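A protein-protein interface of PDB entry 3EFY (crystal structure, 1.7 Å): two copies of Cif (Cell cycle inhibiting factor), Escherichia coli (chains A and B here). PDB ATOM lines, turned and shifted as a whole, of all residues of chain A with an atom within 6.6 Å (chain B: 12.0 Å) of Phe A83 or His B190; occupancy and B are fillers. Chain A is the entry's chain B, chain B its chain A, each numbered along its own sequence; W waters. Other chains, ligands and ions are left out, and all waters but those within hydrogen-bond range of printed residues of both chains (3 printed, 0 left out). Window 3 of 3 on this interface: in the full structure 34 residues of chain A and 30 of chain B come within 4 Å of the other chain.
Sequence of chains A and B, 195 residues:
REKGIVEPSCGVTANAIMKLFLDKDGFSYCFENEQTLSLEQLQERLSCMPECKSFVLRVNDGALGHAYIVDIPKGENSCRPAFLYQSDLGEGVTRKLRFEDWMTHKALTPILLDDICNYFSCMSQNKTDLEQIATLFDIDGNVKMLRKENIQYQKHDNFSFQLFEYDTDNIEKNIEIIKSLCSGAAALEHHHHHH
A ring nitrogen (NE2) of His B190 sits at hydrogen-bond distance from the side-chain carboxylate of Asp A71 (3.3 Å). The side-chain hydroxyl of Tyr A85 lies close to the backbone carbonyl oxygen of Ala B187. A ring nitrogen (NE2) of His B190 sits at hydrogen-bond distance from the side-chain hydroxyl (OH) of Tyr A85, at 2.6 Å.
The side-chain hydroxyl (OH) of Tyr A166 sits at hydrogen-bond distance from the side-chain carboxylate (OD1) of Asp A71 (2.6 Å). The backbone carbonyl oxygen (O) of Ile A69 lies within hydrogen-bond range of the backbone NH (N) of Tyr A85 (2.9 Å). OD2 of Asp A71 is in hydrogen-bond range of OH of Tyr A85 (2.6 Å). N of Asp A71 lies within hydrogen-bond range of O of Phe A83 (2.8 Å).
Phe A21 touches Leu B188. OD2 of Asp A71 touches O of Leu B188 (3.8 Å). Phe A83 touches His B190. Tyr A85 touches Leu B188. Ala B187 touches Leu A108.
Ile A69 touches none of the printed residues of chain B. No residue of chain B comes within 4 Å of Val A70. Of chain B, only Leu B188 and His B190 come within 4 Å of Asp A71. No residue of chain B comes within 4 Å of Pro A73. No residue of chain B comes within 4 Å of Pro A81. No residue of chain B comes within 4 Å of Ala A82. Of chain B, only His B190 comes within 4 Å of Phe A83. No residue of chain B comes within 4 Å of Leu A84. Tyr A85 touches just these residues of chain B: Ala B187, Leu B188 and His B190. Ala A107 touches none of the printed residues of chain B. Printed residues of chain B within 4 Å of Leu A108: Ala B187 (3.6 Å). No residue of chain B comes within 4 Å of Thr A109. No residue of chain B comes within 4 Å of Ile A111. Of the printed residues of chain A, Ala B187 touches Tyr A85 and Leu A108. His B190 touches just these residues of chain A: Asp A71, Phe A83 and Tyr A85.
Printed residues of chain A that touch a printed residue of chain B: Phe A21, Asp A71, Phe A83, Tyr A85 and Leu A108. Hydrophobic or aromatic side chains of chain A within 4 Å of the printed part of chain B: Phe A21, Phe A83, Tyr A85 and Leu A108. Printed residues of chain B that touch a printed residue of chain A: Ala B187, Leu B188 and His B190. Along chain B the printed residues that touch a printed residue of chain A span positions 187 to 190. Among the printed residues, no Asp or Glu carboxylate lies within 4 Å of a Lys or Arg side-chain nitrogen of the other chain.
No position is printed for both chains. Of the 8 pairs that touch across the chains among the printed residues, none has its exchanged pair printed and touching as well.
Water W1 lies within hydrogen-bond range of the backbone carbonyl oxygen (O) of Leu B188, the side-chain carboxylate (OD2) of Asp A71 and the side-chain hydroxyl (OH) of Tyr A166. Water W3 lies within hydrogen-bond range of OE2 of Glu B189 (2.7 Å) and O of Thr A168 (3.0 Å). Water W2 bridges O of Ala B187 and O of Ala A107.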
ATOM      1  N   PHE A  21      30.071  -1.496  24.467  1.00  0.00           N
ATOM      2  CA  PHE A  21      29.726  -2.288  23.290  1.00  0.00           C
ATOM      3  C   PHE A  21      30.637  -2.078  22.093  1.00  0.00           C
ATOM      4  O   PHE A  21      30.853  -3.006  21.314  1.00  0.00           O
ATOM      5  CB  PHE A  21      28.283  -1.995  22.878  1.00  0.00           C
ATOM      6  CG  PHE A  21      27.268  -2.725  23.704  1.00  0.00           C
ATOM      7  CD1 PHE A  21      26.826  -3.982  23.336  1.00  0.00           C
ATOM      8  CD2 PHE A  21      26.755  -2.152  24.873  1.00  0.00           C
ATOM      9  CE1 PHE A  21      25.879  -4.660  24.107  1.00  0.00           C
ATOM     10  CE2 PHE A  21      25.814  -2.807  25.636  1.00  0.00           C
ATOM     11  CZ  PHE A  21      25.412  -4.101  25.271  1.00  0.00           C
ATOM     12  N   ILE A  69      19.546   2.874  26.810  1.00  0.00           N
ATOM     13  CA  ILE A  69      20.089   1.950  25.816  1.00  0.00           C
ATOM     14  C   ILE A  69      19.118   0.800  25.629  1.00  0.00           C
ATOM     15  O   ILE A  69      18.586   0.192  26.617  1.00  0.00           O
ATOM     16  CB  ILE A  69      21.450   1.375  26.254  1.00  0.00           C
ATOM     17  CG1 ILE A  69      22.483   2.462  26.560  1.00  0.00           C
ATOM     18  CG2 ILE A  69      22.006   0.358  25.203  1.00  0.00           C
ATOM     19  CD1 ILE A  69      22.830   3.474  25.475  1.00  0.00           C
ATOM     20  N   VAL A  70      18.899   0.458  24.352  1.00  0.00           N
ATOM     21  CA  VAL A  70      18.116  -0.713  23.989  1.00  0.00           C
ATOM     22  C   VAL A  70      19.085  -1.658  23.276  1.00  0.00           C
ATOM     23  O   VAL A  70      19.709  -1.291  22.274  1.00  0.00           O
ATOM     24  CB  VAL A  70      16.870  -0.382  23.121  1.00  0.00           C
ATOM     25  CG1 VAL A  70      16.146  -1.658  22.687  1.00  0.00           C
ATOM     26  CG2 VAL A  70      15.925   0.588  23.899  1.00  0.00           C
ATOM     27  N   ASP A  71      19.235  -2.855  23.831  1.00  0.00           N
ATOM     28  CA  ASP A  71      20.127  -3.899  23.284  1.00  0.00           C
ATOM     29  C   ASP A  71      19.250  -4.893  22.561  1.00  0.00           C
ATOM     30  O   ASP A  71      18.291  -5.430  23.133  1.00  0.00           O
ATOM     31  CB  ASP A  71      20.917  -4.521  24.455  1.00  0.00           C
ATOM     32  CG  ASP A  71      21.828  -5.659  24.069  1.00  0.00           C
ATOM     33  OD1 ASP A  71      21.848  -6.079  22.894  1.00  0.00           O
ATOM     34  OD2 ASP A  71      22.506  -6.162  25.010  1.00  0.00           O
ATOM     35  N   ILE A  72      19.543  -5.098  21.279  1.00  0.00           N
ATOM     36  CA  ILE A  72      18.809  -6.001  20.413  1.00  0.00           C
ATOM     37  C   ILE A  72      19.750  -7.154  20.016  1.00  0.00           C
ATOM     38  O   ILE A  72      20.477  -7.071  19.023  1.00  0.00           O
ATOM     39  CB  ILE A  72      18.270  -5.278  19.140  1.00  0.00           C
ATOM     40  CG1 ILE A  72      17.429  -4.038  19.477  1.00  0.00           C
ATOM     41  CG2 ILE A  72      17.458  -6.270  18.268  1.00  0.00           C
ATOM     42  CD1 ILE A  72      17.221  -3.084  18.287  1.00  0.00           C
ATOM     43  N   PRO A  73      19.713  -8.252  20.761  1.00  0.00           N
ATOM     44  CA  PRO A  73      20.564  -9.383  20.371  1.00  0.00           C
ATOM     45  C   PRO A  73      20.092 -10.022  19.064  1.00  0.00           C
ATOM     46  O   PRO A  73      19.003  -9.710  18.556  1.00  0.00           O
ATOM     47  CB  PRO A  73      20.399 -10.368  21.539  1.00  0.00           C
ATOM     48  CG  PRO A  73      19.885  -9.513  22.697  1.00  0.00           C
ATOM     49  CD  PRO A  73      19.007  -8.508  22.026  1.00  0.00           C
ATOM     50  N   PRO A  81      13.077  -9.910  20.709  1.00  0.00           N
ATOM     51  CA  PRO A  81      13.369  -9.414  22.062  1.00  0.00           C
ATOM     52  C   PRO A  81      14.401  -8.303  22.116  1.00  0.00           C
ATOM     53  O   PRO A  81      15.210  -8.125  21.176  1.00  0.00           O
ATOM     54  CB  PRO A  81      13.917 -10.637  22.801  1.00  0.00           C
ATOM     55  CG  PRO A  81      13.966 -11.736  21.824  1.00  0.00           C
ATOM     56  CD  PRO A  81      13.649 -11.253  20.465  1.00  0.00           C
ATOM     57  N   ALA A  82      14.350  -7.541  23.198  1.00  0.00           N
ATOM     58  CA  ALA A  82      15.354  -6.534  23.466  1.00  0.00           C
ATOM     59  C   ALA A  82      15.501  -6.395  24.979  1.00  0.00           C
ATOM     60  O   ALA A  82      14.669  -6.908  25.745  1.00  0.00           O
ATOM     61  CB  ALA A  82      14.937  -5.211  22.847  1.00  0.00           C
ATOM     62  N   PHE A  83      16.555  -5.696  25.391  1.00  0.00           N
ATOM     63  CA  PHE A  83      16.840  -5.416  26.803  1.00  0.00           C
ATOM     64  C   PHE A  83      17.043  -3.913  26.943  1.00  0.00           C
ATOM     65  O   PHE A  83      17.562  -3.265  26.028  1.00  0.00           O
ATOM     66  CB  PHE A  83      18.037  -6.183  27.321  1.00  0.00           C
ATOM     67  CG  PHE A  83      17.871  -7.675  27.271  1.00  0.00           C
ATOM     68  CD1 PHE A  83      17.392  -8.338  28.375  1.00  0.00           C
ATOM     69  CD2 PHE A  83      18.153  -8.403  26.130  1.00  0.00           C
ATOM     70  CE1 PHE A  83      17.229  -9.682  28.360  1.00  0.00           C
ATOM     71  CE2 PHE A  83      17.976  -9.765  26.093  1.00  0.00           C
ATOM     72  CZ  PHE A  83      17.497 -10.407  27.214  1.00  0.00           C
ATOM     73  N   LEU A  84      16.567  -3.338  28.057  1.00  0.00           N
ATOM     74  CA  LEU A  84      16.656  -1.938  28.317  1.00  0.00           C
ATOM     75  C   LEU A  84      17.587  -1.690  29.511  1.00  0.00           C
ATOM     76  O   LEU A  84      17.387  -2.293  30.593  1.00  0.00           O
ATOM     77  CB  LEU A  84      15.248  -1.404  28.672  1.00  0.00           C
ATOM     78  CG  LEU A  84      15.143   0.038  29.148  1.00  0.00           C
ATOM     79  CD1 LEU A  84      15.539   0.956  28.031  1.00  0.00           C
ATOM     80  CD2 LEU A  84      13.679   0.337  29.607  1.00  0.00           C
ATOM     81  N   TYR A  85      18.563  -0.813  29.323  1.00  0.00           N
ATOM     82  CA  TYR A  85      19.546  -0.422  30.310  1.00  0.00           C
ATOM     83  C   TYR A  85      19.392   1.074  30.590  1.00  0.00           C
ATOM     84  O   TYR A  85      19.394   1.903  29.673  1.00  0.00           O
ATOM     85  CB  TYR A  85      20.968  -0.728  29.873  1.00  0.00           C
ATOM     86  CG  TYR A  85      21.192  -2.084  29.224  1.00  0.00           C
ATOM     87  CD1 TYR A  85      20.644  -3.242  29.773  1.00  0.00           C
ATOM     88  CD2 TYR A  85      21.978  -2.208  28.076  1.00  0.00           C
ATOM     89  CE1 TYR A  85      20.855  -4.488  29.213  1.00  0.00           C
ATOM     90  CE2 TYR A  85      22.208  -3.442  27.511  1.00  0.00           C
ATOM     91  CZ  TYR A  85      21.633  -4.599  28.055  1.00  0.00           C
ATOM     92  OH  TYR A  85      21.818  -5.852  27.475  1.00  0.00           O
ATOM     93  N   LYS A 106      14.886  -5.410  37.136  1.00  0.00           N
ATOM     94  CA  LYS A 106      14.026  -5.400  35.944  1.00  0.00           C
ATOM     95  C   LYS A 106      14.796  -5.553  34.614  1.00  0.00           C
ATOM     96  O   LYS A 106      14.265  -6.127  33.661  1.00  0.00           O
ATOM     97  CB  LYS A 106      13.156  -4.142  35.940  1.00  0.00           C
ATOM     98  CG  LYS A 106      12.069  -4.145  34.924  1.00  0.00           C
ATOM     99  CD  LYS A 106      10.923  -3.235  35.335  1.00  0.00           C
ATOM    100  CE  LYS A 106       9.911  -3.024  34.248  1.00  0.00           C
ATOM    101  NZ  LYS A 106       8.691  -2.251  34.716  1.00  0.00           N
ATOM    102  N   ALA A 107      16.025  -5.077  34.561  1.00  0.00           N
ATOM    103  CA  ALA A 107      16.821  -5.135  33.287  1.00  0.00           C
ATOM    104  C   ALA A 107      17.022  -6.559  32.829  1.00  0.00           C
ATOM    105  O   ALA A 107      17.228  -6.840  31.655  1.00  0.00           O
ATOM    106  CB  ALA A 107      18.190  -4.485  33.484  1.00  0.00           C
ATOM    107  N   LEU A 108      17.005  -7.508  33.764  1.00  0.00           N
ATOM    108  CA  LEU A 108      17.282  -8.898  33.414  1.00  0.00           C
ATOM    109  C   LEU A 108      16.186  -9.594  32.598  1.00  0.00           C
ATOM    110  O   LEU A 108      16.438 -10.611  31.979  1.00  0.00           O
ATOM    111  CB  LEU A 108      17.570  -9.706  34.699  1.00  0.00           C
ATOM    112  CG  LEU A 108      18.808  -9.262  35.437  1.00  0.00           C
ATOM    113  CD1 LEU A 108      18.805  -9.873  36.834  1.00  0.00           C
ATOM    114  CD2 LEU A 108      20.069  -9.623  34.686  1.00  0.00           C
ATOM    115  N   THR A 109      14.976  -9.059  32.621  1.00  0.00           N
ATOM    116  CA  THR A 109      13.883  -9.639  31.892  1.00  0.00           C
ATOM    117  C   THR A 109      13.779  -8.984  30.494  1.00  0.00           C
ATOM    118  O   THR A 109      13.683  -7.766  30.399  1.00  0.00           O
ATOM    119  CB  THR A 109      12.576  -9.443  32.691  1.00  0.00           C
ATOM    120  OG1 THR A 109      12.685 -10.182  33.935  1.00  0.00           O
ATOM    121  CG2 THR A 109      11.364  -9.946  31.928  1.00  0.00           C
ATOM    122  N   PRO A 110      13.761  -9.803  29.438  1.00  0.00           N
ATOM    123  CA  PRO A 110      13.604  -9.230  28.110  1.00  0.00           C
ATOM    124  C   PRO A 110      12.248  -8.575  27.931  1.00  0.00           C
ATOM    125  O   PRO A 110      11.239  -8.967  28.557  1.00  0.00           O
ATOM    126  CB  PRO A 110      13.776 -10.415  27.181  1.00  0.00           C
ATOM    127  CG  PRO A 110      13.527 -11.588  28.007  1.00  0.00           C
ATOM    128  CD  PRO A 110      13.883 -11.264  29.394  1.00  0.00           C
ATOM    129  N   ILE A 111      12.229  -7.564  27.080  1.00  0.00           N
ATOM    130  CA  ILE A 111      11.021  -6.985  26.594  1.00  0.00           C
ATOM    131  C   ILE A 111      10.871  -7.332  25.100  1.00  0.00           C
ATOM    132  O   ILE A 111      11.762  -7.929  24.501  1.00  0.00           O
ATOM    133  CB  ILE A 111      10.997  -5.464  26.813  1.00  0.00           C
ATOM    134  CG1 ILE A 111      12.113  -4.717  26.076  1.00  0.00           C
ATOM    135  CG2 ILE A 111      11.086  -5.128  28.346  1.00  0.00           C
ATOM    136  CD1 ILE A 111      12.004  -3.156  26.216  1.00  0.00           C
ATOM    137  N   TYR A 166      26.782  -4.402  16.932  1.00  0.00           N
ATOM    138  CA  TYR A 166      27.852  -4.804  17.831  1.00  0.00           C
ATOM    139  C   TYR A 166      28.163  -6.287  17.707  1.00  0.00           C
ATOM    140  O   TYR A 166      27.349  -7.049  17.231  1.00  0.00           O
ATOM    141  CB  TYR A 166      27.581  -4.473  19.304  1.00  0.00           C
ATOM    142  CG  TYR A 166      26.569  -5.329  20.027  1.00  0.00           C
ATOM    143  CD1 TYR A 166      26.948  -6.469  20.707  1.00  0.00           C
ATOM    144  CD2 TYR A 166      25.217  -4.960  20.065  1.00  0.00           C
ATOM    145  CE1 TYR A 166      26.025  -7.248  21.391  1.00  0.00           C
ATOM    146  CE2 TYR A 166      24.300  -5.717  20.729  1.00  0.00           C
ATOM    147  CZ  TYR A 166      24.711  -6.876  21.426  1.00  0.00           C
ATOM    148  OH  TYR A 166      23.745  -7.632  22.099  1.00  0.00           O
ATOM    149  N   THR A 168      29.275  -9.596  20.003  1.00  0.00           N
ATOM    150  CA  THR A 168      29.233 -10.106  21.379  1.00  0.00           C
ATOM    151  C   THR A 168      30.640 -10.259  21.971  1.00  0.00           C
ATOM    152  O   THR A 168      30.816 -10.062  23.172  1.00  0.00           O
ATOM    153  CB  THR A 168      28.436 -11.447  21.493  1.00  0.00           C
ATOM    154  OG1 THR A 168      28.950 -12.368  20.526  1.00  0.00           O
ATOM    155  CG2 THR A 168      26.973 -11.223  21.215  1.00  0.00           C
ATOM    156  N   GLY B 184      26.475  -3.421  37.504  1.00  0.00           N
ATOM    157  CA  GLY B 184      25.394  -3.905  36.659  1.00  0.00           C
ATOM    158  C   GLY B 184      25.784  -4.792  35.486  1.00  0.00           C
ATOM    159  O   GLY B 184      24.970  -5.120  34.652  1.00  0.00           O
ATOM    160  N   ALA B 185      27.050  -5.199  35.415  1.00  0.00           N
ATOM    161  CA  ALA B 185      27.596  -5.799  34.208  1.00  0.00           C
ATOM    162  C   ALA B 185      26.973  -7.115  33.800  1.00  0.00           C
ATOM    163  O   ALA B 185      26.887  -7.395  32.606  1.00  0.00           O
ATOM    164  CB  ALA B 185      29.128  -5.941  34.321  1.00  0.00           C
ATOM    165  N   ALA B 186      26.487  -7.912  34.764  1.00  0.00           N
ATOM    166  CA  ALA B 186      25.895  -9.188  34.421  1.00  0.00           C
ATOM    167  C   ALA B 186      24.710  -9.025  33.446  1.00  0.00           C
ATOM    168  O   ALA B 186      24.472  -9.862  32.595  1.00  0.00           O
ATOM    169  CB  ALA B 186      25.457  -9.957  35.730  1.00  0.00           C
ATOM    170  N   ALA B 187      23.967  -7.936  33.572  1.00  0.00           N
ATOM    171  CA  ALA B 187      22.782  -7.725  32.744  1.00  0.00           C
ATOM    172  C   ALA B 187      23.120  -7.264  31.301  1.00  0.00           C
ATOM    173  O   ALA B 187      22.204  -7.181  30.438  1.00  0.00           O
ATOM    174  CB  ALA B 187      21.844  -6.700  33.417  1.00  0.00           C
ATOM    175  N   LEU B 188      24.388  -6.954  31.037  1.00  0.00           N
ATOM    176  CA  LEU B 188      24.778  -6.422  29.721  1.00  0.00           C
ATOM    177  C   LEU B 188      25.071  -7.506  28.693  1.00  0.00           C
ATOM    178  O   LEU B 188      25.180  -7.192  27.504  1.00  0.00           O
ATOM    179  CB  LEU B 188      26.002  -5.509  29.862  1.00  0.00           C
ATOM    180  CG  LEU B 188      25.842  -4.216  30.614  1.00  0.00           C
ATOM    181  CD1 LEU B 188      27.186  -3.523  30.877  1.00  0.00           C
ATOM    182  CD2 LEU B 188      24.856  -3.310  29.851  1.00  0.00           C
ATOM    183  N   GLU B 189      25.227  -8.767  29.125  1.00  0.00           N
ATOM    184  CA  GLU B 189      25.530  -9.855  28.215  1.00  0.00           C
ATOM    185  C   GLU B 189      24.460 -10.938  28.268  1.00  0.00           C
ATOM    186  O   GLU B 189      23.887 -11.187  29.333  1.00  0.00           O
ATOM    187  CB  GLU B 189      26.889 -10.449  28.538  1.00  0.00           C
ATOM    188  CG  GLU B 189      28.041  -9.479  28.406  1.00  0.00           C
ATOM    189  CD  GLU B 189      29.388 -10.165  28.607  1.00  0.00           C
ATOM    190  OE1 GLU B 189      29.935 -10.102  29.736  1.00  0.00           O
ATOM    191  OE2 GLU B 189      29.866 -10.779  27.627  1.00  0.00           O
ATOM    192  N   HIS B 190      24.217 -11.568  27.112  1.00  0.00           N
ATOM    193  CA  HIS B 190      23.116 -12.547  26.931  1.00  0.00           C
ATOM    194  C   HIS B 190      23.575 -13.897  26.341  1.00  0.00           C
ATOM    195  O   HIS B 190      24.456 -13.920  25.494  1.00  0.00           O
ATOM    196  CB  HIS B 190      22.059 -11.897  26.054  1.00  0.00           C
ATOM    197  CG  HIS B 190      21.673 -10.565  26.576  1.00  0.00           C
ATOM    198  ND1 HIS B 190      20.959 -10.448  27.743  1.00  0.00           N
ATOM    199  CD2 HIS B 190      22.058  -9.311  26.231  1.00  0.00           C
ATOM    200  CE1 HIS B 190      20.856  -9.169  28.056  1.00  0.00           C
ATOM    201  NE2 HIS B 190      21.506  -8.459  27.148  1.00  0.00           N
HETATM  202  O   HOH W   1      24.999  -7.870  25.037  1.00  0.00           O
HETATM  203  O   HOH W   2      19.752  -8.243  31.016  1.00  0.00           O
HETATM  204  O   HOH W   3      28.748 -10.982  25.207  1.00  0.00           O
